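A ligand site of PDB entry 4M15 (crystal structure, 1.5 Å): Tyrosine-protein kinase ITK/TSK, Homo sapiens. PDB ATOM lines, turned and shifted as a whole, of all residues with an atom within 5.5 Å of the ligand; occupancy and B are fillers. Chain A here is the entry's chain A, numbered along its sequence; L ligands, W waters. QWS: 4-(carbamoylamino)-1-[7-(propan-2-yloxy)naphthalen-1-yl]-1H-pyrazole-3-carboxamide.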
ATOM      1  N   TRP A   5      25.767  18.518  21.497  1.00  0.00           N
ATOM      2  CA  TRP A   5      24.778  19.147  22.356  1.00  0.00           C
ATOM      3  C   TRP A   5      25.449  19.723  23.623  1.00  0.00           C
ATOM      4  O   TRP A   5      24.760  20.386  24.395  1.00  0.00           O
ATOM      5  CB  TRP A   5      23.706  18.118  22.717  1.00  0.00           C
ATOM      6  CG  TRP A   5      24.291  16.841  23.214  1.00  0.00           C
ATOM      7  CD1 TRP A   5      24.653  15.749  22.483  1.00  0.00           C
ATOM      8  CD2 TRP A   5      24.683  16.558  24.561  1.00  0.00           C
ATOM      9  NE1 TRP A   5      25.233  14.808  23.286  1.00  0.00           N
ATOM     10  CE2 TRP A   5      25.260  15.268  24.577  1.00  0.00           C
ATOM     11  CE3 TRP A   5      24.561  17.260  25.774  1.00  0.00           C
ATOM     12  CZ2 TRP A   5      25.737  14.673  25.743  1.00  0.00           C
ATOM     13  CZ3 TRP A   5      25.015  16.656  26.941  1.00  0.00           C
ATOM     14  CH2 TRP A   5      25.609  15.389  26.913  1.00  0.00           C
ATOM     15  N   PHE A  52      18.930  12.189  31.535  1.00  0.00           N
ATOM     16  CA  PHE A  52      18.636  13.202  30.535  1.00  0.00           C
ATOM     17  C   PHE A  52      19.693  13.250  29.417  1.00  0.00           C
ATOM     18  O   PHE A  52      19.349  13.134  28.235  1.00  0.00           O
ATOM     19  CB  PHE A  52      18.518  14.550  31.251  1.00  0.00           C
ATOM     20  CG  PHE A  52      18.153  15.702  30.350  1.00  0.00           C
ATOM     21  CD1 PHE A  52      16.825  15.958  30.021  1.00  0.00           C
ATOM     22  CD2 PHE A  52      19.135  16.553  29.850  1.00  0.00           C
ATOM     23  CE1 PHE A  52      16.484  17.052  29.236  1.00  0.00           C
ATOM     24  CE2 PHE A  52      18.789  17.637  29.038  1.00  0.00           C
ATOM     25  CZ  PHE A  52      17.467  17.841  28.719  1.00  0.00           C
ATOM     26  N   ILE A  53      20.963  13.353  29.817  1.00  0.00           N
ATOM     27  CA  ILE A  53      22.107  13.390  28.911  1.00  0.00           C
ATOM     28  C   ILE A  53      22.142  12.169  27.941  1.00  0.00           C
ATOM     29  O   ILE A  53      22.515  12.328  26.769  1.00  0.00           O
ATOM     30  CB  ILE A  53      23.362  13.559  29.825  1.00  0.00           C
ATOM     31  CG1 ILE A  53      23.787  15.035  29.972  1.00  0.00           C
ATOM     32  CG2 ILE A  53      24.509  12.604  29.572  1.00  0.00           C
ATOM     33  CD1 ILE A  53      22.885  15.974  30.706  1.00  0.00           C
ATOM     34  N   GLU A  55      19.705  10.756  26.395  1.00  0.00           N
ATOM     35  CA  GLU A  55      18.762  10.897  25.300  1.00  0.00           C
ATOM     36  C   GLU A  55      19.112  12.106  24.400  1.00  0.00           C
ATOM     37  O   GLU A  55      18.411  12.319  23.419  1.00  0.00           O
ATOM     38  CB  GLU A  55      17.329  11.083  25.847  1.00  0.00           C
ATOM     39  CG  GLU A  55      16.684   9.768  26.286  1.00  0.00           C
ATOM     40  CD  GLU A  55      15.293   9.904  26.871  1.00  0.00           C
ATOM     41  OE1 GLU A  55      14.474  10.671  26.313  1.00  0.00           O
ATOM     42  OE2 GLU A  55      15.021   9.230  27.889  1.00  0.00           O
ATOM     43  N   ALA A  56      20.163  12.877  24.755  1.00  0.00           N
ATOM     44  CA  ALA A  56      20.479  14.108  24.017  1.00  0.00           C
ATOM     45  C   ALA A  56      20.799  13.898  22.554  1.00  0.00           C
ATOM     46  O   ALA A  56      20.337  14.672  21.725  1.00  0.00           O
ATOM     47  CB  ALA A  56      21.630  14.843  24.699  1.00  0.00           C
ATOM     48  N   MET A  59      17.351  13.181  20.901  1.00  0.00           N
ATOM     49  CA  MET A  59      16.420  14.294  20.989  1.00  0.00           C
ATOM     50  C   MET A  59      16.845  15.561  20.276  1.00  0.00           C
ATOM     51  O   MET A  59      15.986  16.355  19.914  1.00  0.00           O
ATOM     52  CB  MET A  59      15.995  14.540  22.456  1.00  0.00           C
ATOM     53  CG  MET A  59      15.302  13.353  23.080  1.00  0.00           C
ATOM     54  SD  MET A  59      13.758  12.947  22.188  1.00  0.00           S
ATOM     55  CE  MET A  59      12.705  13.958  23.026  1.00  0.00           C
ATOM     56  N   MET A  60      18.157  15.741  20.020  1.00  0.00           N
ATOM     57  CA  MET A  60      18.612  16.963  19.303  1.00  0.00           C
ATOM     58  C   MET A  60      18.154  16.993  17.844  1.00  0.00           C
ATOM     59  O   MET A  60      18.202  18.050  17.209  1.00  0.00           O
ATOM     60  CB  MET A  60      20.115  17.220  19.467  1.00  0.00           C
ATOM     61  CG  MET A  60      20.993  16.318  18.659  1.00  0.00           C
ATOM     62  SD  MET A  60      22.734  16.619  19.025  1.00  0.00           S
ATOM     63  CE  MET A  60      22.932  18.314  18.430  1.00  0.00           C
ATOM     64  N   LYS A  61      17.716  15.844  17.331  1.00  0.00           N
ATOM     65  CA  LYS A  61      17.220  15.735  15.958  1.00  0.00           C
ATOM     66  C   LYS A  61      15.812  16.335  15.808  1.00  0.00           C
ATOM     67  O   LYS A  61      15.393  16.577  14.669  1.00  0.00           O
ATOM     68  CB  LYS A  61      17.273  14.276  15.476  1.00  0.00           C
ATOM     69  CG  LYS A  61      18.707  13.771  15.281  1.00  0.00           C
ATOM     70  CD  LYS A  61      18.756  12.252  15.170  1.00  0.00           C
ATOM     71  CE  LYS A  61      20.118  11.706  15.495  1.00  0.00           C
ATOM     72  NZ  LYS A  61      20.064  10.244  15.771  1.00  0.00           N
ATOM     73  N   LEU A  62      15.068  16.546  16.925  1.00  0.00           N
ATOM     74  CA  LEU A  62      13.713  17.102  16.833  1.00  0.00           C
ATOM     75  C   LEU A  62      13.813  18.564  16.493  1.00  0.00           C
ATOM     76  O   LEU A  62      14.537  19.300  17.177  1.00  0.00           O
ATOM     77  CB  LEU A  62      12.897  16.900  18.123  1.00  0.00           C
ATOM     78  CG  LEU A  62      12.623  15.467  18.604  1.00  0.00           C
ATOM     79  CD1 LEU A  62      12.081  15.497  19.992  1.00  0.00           C
ATOM     80  CD2 LEU A  62      11.633  14.745  17.728  1.00  0.00           C
ATOM     81  N   VAL A  68       9.779  24.860  20.774  1.00  0.00           N
ATOM     82  CA  VAL A  68      10.923  25.638  21.292  1.00  0.00           C
ATOM     83  C   VAL A  68      12.157  24.731  21.213  1.00  0.00           C
ATOM     84  O   VAL A  68      12.155  23.641  21.807  1.00  0.00           O
ATOM     85  CB  VAL A  68      10.673  26.090  22.747  1.00  0.00           C
ATOM     86  CG1 VAL A  68      11.905  26.800  23.325  1.00  0.00           C
ATOM     87  CG2 VAL A  68       9.451  27.016  22.853  1.00  0.00           C
ATOM     88  N   GLN A  69      13.231  25.207  20.551  1.00  0.00           N
ATOM     89  CA  GLN A  69      14.423  24.377  20.474  1.00  0.00           C
ATOM     90  C   GLN A  69      15.237  24.422  21.779  1.00  0.00           C
ATOM     91  O   GLN A  69      15.503  25.520  22.309  1.00  0.00           O
ATOM     92  CB  GLN A  69      15.311  24.827  19.305  1.00  0.00           C
ATOM     93  CG  GLN A  69      16.309  23.734  18.911  1.00  0.00           C
ATOM     94  CD  GLN A  69      16.982  23.885  17.561  1.00  0.00           C
ATOM     95  OE1 GLN A  69      16.680  24.794  16.766  1.00  0.00           O
ATOM     96  NE2 GLN A  69      17.937  23.012  17.311  1.00  0.00           N
ATOM     97  N   LEU A  70      15.646  23.238  22.257  1.00  0.00           N
ATOM     98  CA  LEU A  70      16.601  23.102  23.360  1.00  0.00           C
ATOM     99  C   LEU A  70      17.937  22.791  22.665  1.00  0.00           C
ATOM    100  O   LEU A  70      18.127  21.694  22.111  1.00  0.00           O
ATOM    101  CB  LEU A  70      16.174  21.972  24.319  1.00  0.00           C
ATOM    102  CG  LEU A  70      17.115  21.643  25.489  1.00  0.00           C
ATOM    103  CD1 LEU A  70      17.611  22.864  26.210  1.00  0.00           C
ATOM    104  CD2 LEU A  70      16.414  20.715  26.481  1.00  0.00           C
ATOM    105  N   TYR A  71      18.819  23.807  22.574  1.00  0.00           N
ATOM    106  CA  TYR A  71      20.059  23.716  21.831  1.00  0.00           C
ATOM    107  C   TYR A  71      21.111  22.816  22.411  1.00  0.00           C
ATOM    108  O   TYR A  71      21.892  22.214  21.678  1.00  0.00           O
ATOM    109  CB  TYR A  71      20.646  25.098  21.636  1.00  0.00           C
ATOM    110  CG  TYR A  71      19.766  26.039  20.855  1.00  0.00           C
ATOM    111  CD1 TYR A  71      19.384  25.735  19.542  1.00  0.00           C
ATOM    112  CD2 TYR A  71      19.429  27.293  21.357  1.00  0.00           C
ATOM    113  CE1 TYR A  71      18.643  26.655  18.776  1.00  0.00           C
ATOM    114  CE2 TYR A  71      18.711  28.210  20.598  1.00  0.00           C
ATOM    115  CZ  TYR A  71      18.312  27.883  19.315  1.00  0.00           C
ATOM    116  OH  TYR A  71      17.606  28.793  18.571  1.00  0.00           O
ATOM    117  N   GLY A  72      21.221  22.845  23.726  1.00  0.00           N
ATOM    118  CA  GLY A  72      22.248  22.050  24.378  1.00  0.00           C
ATOM    119  C   GLY A  72      22.281  22.215  25.877  1.00  0.00           C
ATOM    120  O   GLY A  72      21.434  22.912  26.449  1.00  0.00           O
ATOM    121  N   VAL A  73      23.304  21.614  26.489  1.00  0.00           N
ATOM    122  CA  VAL A  73      23.449  21.628  27.947  1.00  0.00           C
ATOM    123  C   VAL A  73      24.853  22.049  28.300  1.00  0.00           C
ATOM    124  O   VAL A  73      25.806  21.545  27.710  1.00  0.00           O
ATOM    125  CB  VAL A  73      23.142  20.212  28.519  1.00  0.00           C
ATOM    126  CG1 VAL A  73      23.288  20.180  30.050  1.00  0.00           C
ATOM    127  CG2 VAL A  73      21.751  19.717  28.092  1.00  0.00           C
ATOM    128  N   PHE A  84      18.051  27.306  25.667  1.00  0.00           N
ATOM    129  CA  PHE A  84      16.881  27.251  24.796  1.00  0.00           C
ATOM    130  C   PHE A  84      16.810  28.430  23.850  1.00  0.00           C
ATOM    131  O   PHE A  84      17.359  29.514  24.104  1.00  0.00           O
ATOM    132  CB  PHE A  84      15.596  27.344  25.660  1.00  0.00           C
ATOM    133  CG  PHE A  84      15.309  26.177  26.571  1.00  0.00           C
ATOM    134  CD1 PHE A  84      14.511  25.121  26.161  1.00  0.00           C
ATOM    135  CD2 PHE A  84      15.788  26.172  27.887  1.00  0.00           C
ATOM    136  CE1 PHE A  84      14.210  24.057  27.024  1.00  0.00           C
ATOM    137  CE2 PHE A  84      15.511  25.092  28.751  1.00  0.00           C
ATOM    138  CZ  PHE A  84      14.713  24.047  28.319  1.00  0.00           C
ATOM    139  N   VAL A 147       5.533  24.861  21.590  1.00  0.00           N
ATOM    140  CA  VAL A 147       5.461  23.948  22.727  1.00  0.00           C
ATOM    141  C   VAL A 147       6.883  23.727  23.287  1.00  0.00           C
ATOM    142  O   VAL A 147       7.851  23.615  22.532  1.00  0.00           O
ATOM    143  CB  VAL A 147       4.836  22.602  22.283  1.00  0.00           C
ATOM    144  CG1 VAL A 147       4.709  21.608  23.439  1.00  0.00           C
ATOM    145  CG2 VAL A 147       3.466  22.817  21.610  1.00  0.00           C
ATOM    146  N   SER A 148       6.983  23.594  24.626  1.00  0.00           N
ATOM    147  CA  SER A 148       8.272  23.361  25.287  1.00  0.00           C
ATOM    148  C   SER A 148       8.105  22.344  26.423  1.00  0.00           C
ATOM    149  O   SER A 148       6.981  22.008  26.822  1.00  0.00           O
ATOM    150  CB  SER A 148       8.760  24.676  25.881  1.00  0.00           C
ATOM    151  OG  SER A 148      10.093  24.573  26.378  1.00  0.00           O
ATOM    152  N   ASP A 149       9.237  21.769  26.891  1.00  0.00           N
ATOM    153  CA  ASP A 149       9.252  20.909  28.067  1.00  0.00           C
ATOM    154  C   ASP A 149       8.663  19.506  27.882  1.00  0.00           C
ATOM    155  O   ASP A 149       8.415  18.776  28.839  1.00  0.00           O
ATOM    156  CB  ASP A 149       8.633  21.625  29.303  1.00  0.00           C
ATOM    157  CG  ASP A 149       9.388  22.826  29.833  1.00  0.00           C
ATOM    158  OD1 ASP A 149      10.271  23.356  29.105  1.00  0.00           O
ATOM    159  OD2 ASP A 149       9.056  23.302  30.939  1.00  0.00           O
ATOM    160  N   PHE A 150       8.509  19.087  26.632  1.00  0.00           N
ATOM    161  CA  PHE A 150       7.982  17.757  26.350  1.00  0.00           C
ATOM    162  C   PHE A 150       8.938  16.700  26.875  1.00  0.00           C
ATOM    163  O   PHE A 150      10.159  16.853  26.748  1.00  0.00           O
ATOM    164  CB  PHE A 150       7.753  17.567  24.846  1.00  0.00           C
ATOM    165  CG  PHE A 150       8.725  18.229  23.904  1.00  0.00           C
ATOM    166  CD1 PHE A 150       9.821  17.524  23.403  1.00  0.00           C
ATOM    167  CD2 PHE A 150       8.539  19.544  23.503  1.00  0.00           C
ATOM    168  CE1 PHE A 150      10.706  18.138  22.493  1.00  0.00           C
ATOM    169  CE2 PHE A 150       9.419  20.162  22.600  1.00  0.00           C
ATOM    170  CZ  PHE A 150      10.480  19.443  22.078  1.00  0.00           C
ATOM    171  N   GLY A 151       8.376  15.707  27.558  1.00  0.00           N
ATOM    172  CA  GLY A 151       9.148  14.594  28.094  1.00  0.00           C
ATOM    173  C   GLY A 151       9.900  14.875  29.386  1.00  0.00           C
ATOM    174  O   GLY A 151      10.398  13.930  30.020  1.00  0.00           O
ATOM    175  N   MET A 152       9.920  16.137  29.851  1.00  0.00           N
ATOM    176  CA  MET A 152      10.699  16.490  31.046  1.00  0.00           C
ATOM    177  C   MET A 152      10.283  15.834  32.339  1.00  0.00           C
ATOM    178  O   MET A 152      11.140  15.643  33.232  1.00  0.00           O
ATOM    179  CB  MET A 152      10.754  18.014  31.212  1.00  0.00           C
ATOM    180  CG  MET A 152      11.487  18.718  30.085  1.00  0.00           C
ATOM    181  SD  MET A 152      13.222  18.227  29.902  1.00  0.00           S
ATOM    182  CE  MET A 152      13.935  19.085  31.287  1.00  0.00           C
ATOM    183  N   ARG A 154       9.812  12.870  32.930  1.00  0.00           N
ATOM    184  CA  ARG A 154      10.482  11.573  33.074  1.00  0.00           C
ATOM    185  C   ARG A 154      11.799  11.751  33.831  1.00  0.00           C
ATOM    186  O   ARG A 154      12.379  10.750  34.249  1.00  0.00           O
ATOM    187  CB  ARG A 154      10.798  10.960  31.720  1.00  0.00           C
ATOM    188  CG  ARG A 154       9.527  10.524  31.006  1.00  0.00           C
ATOM    189  CD  ARG A 154       9.807   9.666  29.795  1.00  0.00           C
ATOM    190  NE  ARG A 154      10.361  10.446  28.699  1.00  0.00           N
ATOM    191  CZ  ARG A 154      11.596  10.339  28.240  1.00  0.00           C
ATOM    192  NH1 ARG A 154      12.428   9.465  28.777  1.00  0.00           N
ATOM    193  NH2 ARG A 154      12.005  11.115  27.245  1.00  0.00           N
ATOM    194  N   PHE A 155      12.269  12.992  34.005  1.00  0.00           N
ATOM    195  CA  PHE A 155      13.561  13.229  34.660  1.00  0.00           C
ATOM    196  C   PHE A 155      13.422  13.973  35.977  1.00  0.00           C
ATOM    197  O   PHE A 155      14.416  14.079  36.711  1.00  0.00           O
ATOM    198  CB  PHE A 155      14.472  14.065  33.702  1.00  0.00           C
ATOM    199  CG  PHE A 155      14.575  13.415  32.337  1.00  0.00           C
ATOM    200  CD1 PHE A 155      15.402  12.306  32.143  1.00  0.00           C
ATOM    201  CD2 PHE A 155      13.784  13.842  31.273  1.00  0.00           C
ATOM    202  CE1 PHE A 155      15.443  11.658  30.913  1.00  0.00           C
ATOM    203  CE2 PHE A 155      13.841  13.195  30.043  1.00  0.00           C
ATOM    204  CZ  PHE A 155      14.651  12.099  29.870  1.00  0.00           C
HETATM  205  N1  QWS L   1      13.868  17.824  24.519  1.00  0.00           N
HETATM  206  N2  QWS L   1      14.386  17.953  23.270  1.00  0.00           N
HETATM  207  C3  QWS L   1      14.051  19.188  22.880  1.00  0.00           C
HETATM  208  C4  QWS L   1      13.316  19.848  23.893  1.00  0.00           C
HETATM  209  C5  QWS L   1      13.192  18.941  24.938  1.00  0.00           C
HETATM  210  N6  QWS L   1      12.814  21.167  23.804  1.00  0.00           N
HETATM  211  C7  QWS L   1      12.132  21.792  24.840  1.00  0.00           C
HETATM  212  N8  QWS L   1      11.773  23.082  24.497  1.00  0.00           N
HETATM  213  O9  QWS L   1      11.886  21.286  25.932  1.00  0.00           O
HETATM  214  C10 QWS L   1      14.428  19.738  21.593  1.00  0.00           C
HETATM  215  N11 QWS L   1      15.109  18.884  20.762  1.00  0.00           N
HETATM  216  O12 QWS L   1      14.164  20.892  21.258  1.00  0.00           O
HETATM  217  C13 QWS L   1      14.094  16.676  25.314  1.00  0.00           C
HETATM  218  C14 QWS L   1      12.994  15.989  25.797  1.00  0.00           C
HETATM  219  C15 QWS L   1      13.190  14.833  26.529  1.00  0.00           C
HETATM  220  C16 QWS L   1      14.481  14.403  26.776  1.00  0.00           C
HETATM  221  C17 QWS L   1      15.402  16.260  25.581  1.00  0.00           C
HETATM  222  C18 QWS L   1      15.575  15.096  26.328  1.00  0.00           C
HETATM  223  C19 QWS L   1      16.849  14.646  26.647  1.00  0.00           C
HETATM  224  C20 QWS L   1      17.938  15.355  26.199  1.00  0.00           C
HETATM  225  C21 QWS L   1      17.776  16.512  25.452  1.00  0.00           C
HETATM  226  C22 QWS L   1      16.508  16.971  25.147  1.00  0.00           C
HETATM  227  O23 QWS L   1      18.947  17.156  25.070  1.00  0.00           O
HETATM  228  C24 QWS L   1      18.778  18.311  24.218  1.00  0.00           C
HETATM  229  C25 QWS L   1      20.123  19.007  24.243  1.00  0.00           C
HETATM  230  C26 QWS L   1      18.535  17.965  22.773  1.00  0.00           C
HETATM  231  O   HOH W   1      16.638  20.046  18.543  1.00  0.00           O
HETATM  232  O   HOH W   2      12.984  21.265  28.543  1.00  0.00           O
HETATM  233  O   HOH W   3      13.262  21.258  18.754  1.00  0.00           O
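Water W3 bridges O12 of the ligand (2.7 Å) and O of Leu 62 (2.8 Å). Water W1 lies within hydrogen-bond range of the backbone carbonyl oxygen (O) of Leu 62 (2.6 Å), the backbone carbonyl oxygen (O) of Met 60 (2.9 Å), a nitrogen (N11) of the ligand (2.9 Å) and the side-chain amide nitrogen (NE2) of Gln 69 (3.5 Å).
The backbone NH of Val 68 lies within hydrogen-bond range of the backbone carbonyl oxygen of Val 147, at 2.9 Å. The side-chain carboxylate (OD1) of Asp 149 is in hydrogen-bond range of the side-chain hydroxyl (OG) of Ser 148 (3.0 Å). NH2 of Arg 154 lies within salt-bridge range of OE1 of Glu 55, 2.7 Å away. The backbone carbonyl oxygen (O) of Trp 5 is in hydrogen-bond range of the backbone NH (N) of Val 73.
O of Val 68 sits at hydrogen-bond distance from N8 of the ligand. O of Met 59 lies within hydrogen-bond range of N11 of the ligand (2.8 Å). The backbone NH (N) of Asp 149 sits at hydrogen-bond distance from an oxygen (O9) of the ligand (2.9 Å). The side-chain hydroxyl of Ser 148 lies within hydrogen-bond range of a nitrogen (N8) of the ligand, 2.9 Å away. N of Leu 70 lies within hydrogen-bond range of O12 of the ligand.
Residues that only touch the ligand: Phe 150, Phe 52, Phe 155, Met 60, Ala 56, Gln 69, Phe 84, Leu 62, Glu 55, Gly 72, Arg 154 and Trp 5. Hydrophobic or aromatic side chains that line the ligand: Trp 5, Phe 52, Ala 56, Met 59, Met 60, Leu 62, Val 68, Leu 70, Phe 84, Phe 150 and Phe 155. Of the 24 residues printed, 17 come within 4 Å of the ligand. The nearest printed residue that does not touch the ligand is Val 73 (4.2 Å).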
